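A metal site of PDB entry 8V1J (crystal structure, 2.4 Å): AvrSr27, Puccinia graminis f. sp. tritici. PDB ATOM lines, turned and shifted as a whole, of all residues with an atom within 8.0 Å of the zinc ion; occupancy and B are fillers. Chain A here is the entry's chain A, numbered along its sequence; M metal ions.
The backbone carbonyl oxygen (O) of Ser 111 is in hydrogen-bond range of a ring nitrogen (ND1) of His 115, 2.9 Å away. N of Ser 13 sits close to SG of Cys 11. N of Cys 11 lies within hydrogen-bond range of OG of Ser 116. The backbone NH of Ser 42 sits close to the side-chain sulfur of Cys 40 (3.4 Å). The side-chain sulfur (SG) of Cys 40 sits close to the backbone NH (N) of Ser 15 (3.5 Å). The backbone carbonyl oxygen of Lys 45 is in hydrogen-bond range of the backbone NH of Cys 40 (3.1 Å).
Four residues have an atom within 4 Å of the zinc ion: Cys 11, Cys 40, Cys 43 and His 115. The nearest printed residue that does not touch the zinc ion is Ser 42 (4.3 Å).
The zinc ion is bound by NE2 of His 115 (2.1 Å), SG of Cys 11 (2.3 Å), SG of Cys 43 (2.3 Å) and SG of Cys 40 (2.3 Å). The zinc ion has four donor atoms within binding distance.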
ATOM      1  N   ASN A  10      30.071 -20.613  23.610  1.00  0.00           N
ATOM      2  CA  ASN A  10      29.251 -21.352  24.549  1.00  0.00           C
ATOM      3  C   ASN A  10      29.283 -20.707  25.938  1.00  0.00           C
ATOM      4  O   ASN A  10      30.147 -19.890  26.248  1.00  0.00           O
ATOM      5  CB  ASN A  10      29.717 -22.808  24.651  1.00  0.00           C
ATOM      6  CG  ASN A  10      29.524 -23.570  23.355  1.00  0.00           C
ATOM      7  OD1 ASN A  10      28.642 -23.246  22.557  1.00  0.00           O
ATOM      8  ND2 ASN A  10      30.336 -24.597  23.152  1.00  0.00           N
ATOM      9  N   CYS A  11      28.318 -21.095  26.771  1.00  0.00           N
ATOM     10  CA  CYS A  11      28.260 -20.688  28.158  1.00  0.00           C
ATOM     11  C   CYS A  11      28.890 -21.779  29.016  1.00  0.00           C
ATOM     12  O   CYS A  11      28.430 -22.928  28.995  1.00  0.00           O
ATOM     13  CB  CYS A  11      26.820 -20.435  28.595  1.00  0.00           C
ATOM     14  SG  CYS A  11      26.558 -20.402  30.381  1.00  0.00           S
ATOM     15  N   ASN A  12      29.928 -21.426  29.770  1.00  0.00           N
ATOM     16  CA  ASN A  12      30.698 -22.398  30.533  1.00  0.00           C
ATOM     17  C   ASN A  12      30.293 -22.445  32.005  1.00  0.00           C
ATOM     18  O   ASN A  12      30.953 -23.139  32.792  1.00  0.00           O
ATOM     19  CB  ASN A  12      32.189 -22.072  30.419  1.00  0.00           C
ATOM     20  CG  ASN A  12      32.636 -21.872  28.989  1.00  0.00           C
ATOM     21  OD1 ASN A  12      32.991 -20.763  28.584  1.00  0.00           O
ATOM     22  ND2 ASN A  12      32.605 -22.942  28.196  1.00  0.00           N
ATOM     23  N   SER A  13      29.237 -21.740  32.388  1.00  0.00           N
ATOM     24  CA  SER A  13      28.736 -21.748  33.767  1.00  0.00           C
ATOM     25  C   SER A  13      27.234 -21.977  33.748  1.00  0.00           C
ATOM     26  O   SER A  13      26.437 -21.065  34.022  1.00  0.00           O
ATOM     27  CB  SER A  13      29.087 -20.442  34.487  1.00  0.00           C
ATOM     28  OG  SER A  13      30.447 -20.426  34.848  1.00  0.00           O
ATOM     29  N   PRO A  14      26.795 -23.191  33.424  1.00  0.00           N
ATOM     30  CA  PRO A  14      25.360 -23.502  33.510  1.00  0.00           C
ATOM     31  C   PRO A  14      24.859 -23.351  34.942  1.00  0.00           C
ATOM     32  O   PRO A  14      25.437 -23.889  35.882  1.00  0.00           O
ATOM     33  CB  PRO A  14      25.277 -24.951  33.022  1.00  0.00           C
ATOM     34  CG  PRO A  14      26.669 -25.487  33.097  1.00  0.00           C
ATOM     35  CD  PRO A  14      27.574 -24.324  32.876  1.00  0.00           C
ATOM     36  N   SER A  15      23.775 -22.596  35.090  1.00  0.00           N
ATOM     37  CA  SER A  15      23.115 -22.379  36.384  1.00  0.00           C
ATOM     38  C   SER A  15      21.614 -22.393  36.106  1.00  0.00           C
ATOM     39  O   SER A  15      21.049 -21.395  35.657  1.00  0.00           O
ATOM     40  CB  SER A  15      23.558 -21.066  37.016  1.00  0.00           C
ATOM     41  OG  SER A  15      22.834 -20.810  38.212  1.00  0.00           O
ATOM     42  N   LEU A  16      20.971 -23.525  36.406  1.00  0.00           N
ATOM     43  CA  LEU A  16      19.655 -23.826  35.852  1.00  0.00           C
ATOM     44  C   LEU A  16      18.530 -23.387  36.778  1.00  0.00           C
ATOM     45  O   LEU A  16      18.644 -23.472  38.002  1.00  0.00           O
ATOM     46  CB  LEU A  16      19.534 -25.325  35.557  1.00  0.00           C
ATOM     47  CG  LEU A  16      19.806 -25.764  34.120  1.00  0.00           C
ATOM     48  CD1 LEU A  16      21.084 -25.148  33.567  1.00  0.00           C
ATOM     49  CD2 LEU A  16      19.873 -27.278  34.043  1.00  0.00           C
ATOM     50  N   SER A  39      15.905 -23.036  32.123  1.00  0.00           N
ATOM     51  CA  SER A  39      16.638 -21.847  31.734  1.00  0.00           C
ATOM     52  C   SER A  39      17.976 -21.791  32.467  1.00  0.00           C
ATOM     53  O   SER A  39      18.076 -22.188  33.628  1.00  0.00           O
ATOM     54  CB  SER A  39      15.847 -20.569  32.033  1.00  0.00           C
ATOM     55  OG  SER A  39      14.619 -20.562  31.319  1.00  0.00           O
ATOM     56  N   CYS A  40      18.985 -21.295  31.770  1.00  0.00           N
ATOM     57  CA  CYS A  40      20.268 -20.972  32.382  1.00  0.00           C
ATOM     58  C   CYS A  40      20.288 -19.478  32.664  1.00  0.00           C
ATOM     59  O   CYS A  40      20.201 -18.661  31.742  1.00  0.00           O
ATOM     60  CB  CYS A  40      21.430 -21.356  31.479  1.00  0.00           C
ATOM     61  SG  CYS A  40      23.053 -20.855  32.130  1.00  0.00           S
ATOM     62  N   THR A  41      20.406 -19.119  33.943  1.00  0.00           N
ATOM     63  CA  THR A  41      20.446 -17.703  34.311  1.00  0.00           C
ATOM     64  C   THR A  41      21.708 -17.015  33.831  1.00  0.00           C
ATOM     65  O   THR A  41      21.700 -15.800  33.647  1.00  0.00           O
ATOM     66  CB  THR A  41      20.301 -17.558  35.828  1.00  0.00           C
ATOM     67  OG1 THR A  41      21.347 -18.284  36.477  1.00  0.00           O
ATOM     68  CG2 THR A  41      18.953 -18.094  36.297  1.00  0.00           C
ATOM     69  N   SER A  42      22.789 -17.774  33.604  1.00  0.00           N
ATOM     70  CA  SER A  42      24.042 -17.161  33.193  1.00  0.00           C
ATOM     71  C   SER A  42      23.969 -16.651  31.757  1.00  0.00           C
ATOM     72  O   SER A  42      24.386 -15.529  31.463  1.00  0.00           O
ATOM     73  CB  SER A  42      25.188 -18.156  33.349  1.00  0.00           C
ATOM     74  OG  SER A  42      25.311 -18.602  34.692  1.00  0.00           O
ATOM     75  N   CYS A  43      23.441 -17.477  30.842  1.00  0.00           N
ATOM     76  CA  CYS A  43      23.359 -17.127  29.439  1.00  0.00           C
ATOM     77  C   CYS A  43      21.939 -16.831  28.963  1.00  0.00           C
ATOM     78  O   CYS A  43      21.769 -16.343  27.839  1.00  0.00           O
ATOM     79  CB  CYS A  43      23.947 -18.260  28.575  1.00  0.00           C
ATOM     80  SG  CYS A  43      22.994 -19.796  28.581  1.00  0.00           S
ATOM     81  N   ARG A  44      20.924 -17.104  29.780  1.00  0.00           N
ATOM     82  CA  ARG A  44      19.542 -16.696  29.504  1.00  0.00           C
ATOM     83  C   ARG A  44      18.969 -17.381  28.267  1.00  0.00           C
ATOM     84  O   ARG A  44      18.103 -16.825  27.575  1.00  0.00           O
ATOM     85  CB  ARG A  44      19.436 -15.170  29.382  1.00  0.00           C
ATOM     86  CG  ARG A  44      19.088 -14.525  30.700  1.00  0.00           C
ATOM     87  CD  ARG A  44      19.414 -13.040  30.769  1.00  0.00           C
ATOM     88  NE  ARG A  44      18.393 -12.177  30.185  1.00  0.00           N
ATOM     89  CZ  ARG A  44      17.141 -12.073  30.632  1.00  0.00           C
ATOM     90  NH1 ARG A  44      16.722 -12.814  31.646  1.00  0.00           N
ATOM     91  NH2 ARG A  44      16.288 -11.248  30.046  1.00  0.00           N
ATOM     92  N   LYS A  45      19.413 -18.596  27.974  1.00  0.00           N
ATOM     93  CA  LYS A  45      18.783 -19.426  26.959  1.00  0.00           C
ATOM     94  C   LYS A  45      17.883 -20.453  27.638  1.00  0.00           C
ATOM     95  O   LYS A  45      18.099 -20.821  28.796  1.00  0.00           O
ATOM     96  CB  LYS A  45      19.838 -20.127  26.094  1.00  0.00           C
ATOM     97  CG  LYS A  45      20.887 -19.173  25.531  1.00  0.00           C
ATOM     98  CD  LYS A  45      21.654 -19.773  24.375  1.00  0.00           C
ATOM     99  CE  LYS A  45      22.838 -18.893  23.965  1.00  0.00           C
ATOM    100  NZ  LYS A  45      24.062 -19.185  24.763  1.00  0.00           N
ATOM    101  N   SER A 110      22.412 -30.066  30.149  1.00  0.00           N
ATOM    102  CA  SER A 110      22.886 -28.828  30.760  1.00  0.00           C
ATOM    103  C   SER A 110      24.348 -28.537  30.478  1.00  0.00           C
ATOM    104  O   SER A 110      24.862 -27.515  30.956  1.00  0.00           O
ATOM    105  CB  SER A 110      22.659 -28.880  32.269  1.00  0.00           C
ATOM    106  OG  SER A 110      23.498 -29.844  32.877  1.00  0.00           O
ATOM    107  N   SER A 111      25.040 -29.394  29.734  1.00  0.00           N
ATOM    108  CA  SER A 111      26.449 -29.163  29.472  1.00  0.00           C
ATOM    109  C   SER A 111      26.630 -27.845  28.717  1.00  0.00           C
ATOM    110  O   SER A 111      25.717 -27.389  28.030  1.00  0.00           O
ATOM    111  CB  SER A 111      27.049 -30.312  28.662  1.00  0.00           C
ATOM    112  OG  SER A 111      26.664 -30.237  27.297  1.00  0.00           O
ATOM    113  N   PRO A 112      27.801 -27.206  28.843  1.00  0.00           N
ATOM    114  CA  PRO A 112      28.050 -26.022  28.007  1.00  0.00           C
ATOM    115  C   PRO A 112      27.759 -26.249  26.535  1.00  0.00           C
ATOM    116  O   PRO A 112      27.128 -25.409  25.884  1.00  0.00           O
ATOM    117  CB  PRO A 112      29.545 -25.749  28.256  1.00  0.00           C
ATOM    118  CG  PRO A 112      29.778 -26.253  29.632  1.00  0.00           C
ATOM    119  CD  PRO A 112      28.902 -27.468  29.784  1.00  0.00           C
ATOM    120  N   HIS A 115      23.489 -26.995  26.175  1.00  0.00           N
ATOM    121  CA  HIS A 115      22.546 -25.984  26.636  1.00  0.00           C
ATOM    122  C   HIS A 115      22.726 -24.653  25.915  1.00  0.00           C
ATOM    123  O   HIS A 115      21.782 -23.863  25.845  1.00  0.00           O
ATOM    124  CB  HIS A 115      22.663 -25.799  28.153  1.00  0.00           C
ATOM    125  CG  HIS A 115      23.483 -24.615  28.577  1.00  0.00           C
ATOM    126  ND1 HIS A 115      24.826 -24.705  28.846  1.00  0.00           N
ATOM    127  CD2 HIS A 115      23.131 -23.327  28.793  1.00  0.00           C
ATOM    128  CE1 HIS A 115      25.277 -23.516  29.205  1.00  0.00           C
ATOM    129  NE2 HIS A 115      24.268 -22.656  29.184  1.00  0.00           N
ATOM    130  N   SER A 116      23.916 -24.402  25.345  1.00  0.00           N
ATOM    131  CA  SER A 116      24.143 -23.181  24.581  1.00  0.00           C
ATOM    132  C   SER A 116      23.336 -23.149  23.291  1.00  0.00           C
ATOM    133  O   SER A 116      23.145 -22.064  22.712  1.00  0.00           O
ATOM    134  CB  SER A 116      25.628 -23.024  24.259  1.00  0.00           C
ATOM    135  OG  SER A 116      26.400 -22.848  25.439  1.00  0.00           O
ATOM    136  N   TRP A 118      20.159 -24.286  23.167  1.00  0.00           N
ATOM    137  CA  TRP A 118      18.747 -24.168  23.514  1.00  0.00           C
ATOM    138  C   TRP A 118      18.131 -22.981  22.777  1.00  0.00           C
ATOM    139  O   TRP A 118      18.779 -21.963  22.547  1.00  0.00           O
ATOM    140  CB  TRP A 118      18.579 -23.985  25.016  1.00  0.00           C
ATOM    141  CG  TRP A 118      18.847 -25.200  25.832  1.00  0.00           C
ATOM    142  CD1 TRP A 118      19.022 -26.480  25.371  1.00  0.00           C
ATOM    143  CD2 TRP A 118      18.962 -25.269  27.254  1.00  0.00           C
ATOM    144  NE1 TRP A 118      19.241 -27.336  26.431  1.00  0.00           N
ATOM    145  CE2 TRP A 118      19.207 -26.610  27.601  1.00  0.00           C
ATOM    146  CE3 TRP A 118      18.889 -24.312  28.281  1.00  0.00           C
ATOM    147  CZ2 TRP A 118      19.379 -27.026  28.914  1.00  0.00           C
ATOM    148  CZ3 TRP A 118      19.051 -24.734  29.587  1.00  0.00           C
ATOM    149  CH2 TRP A 118      19.299 -26.074  29.898  1.00  0.00           C
HETATM  150 ZN    ZN M   1      24.309 -20.840  30.160  1.00  0.00          ZN
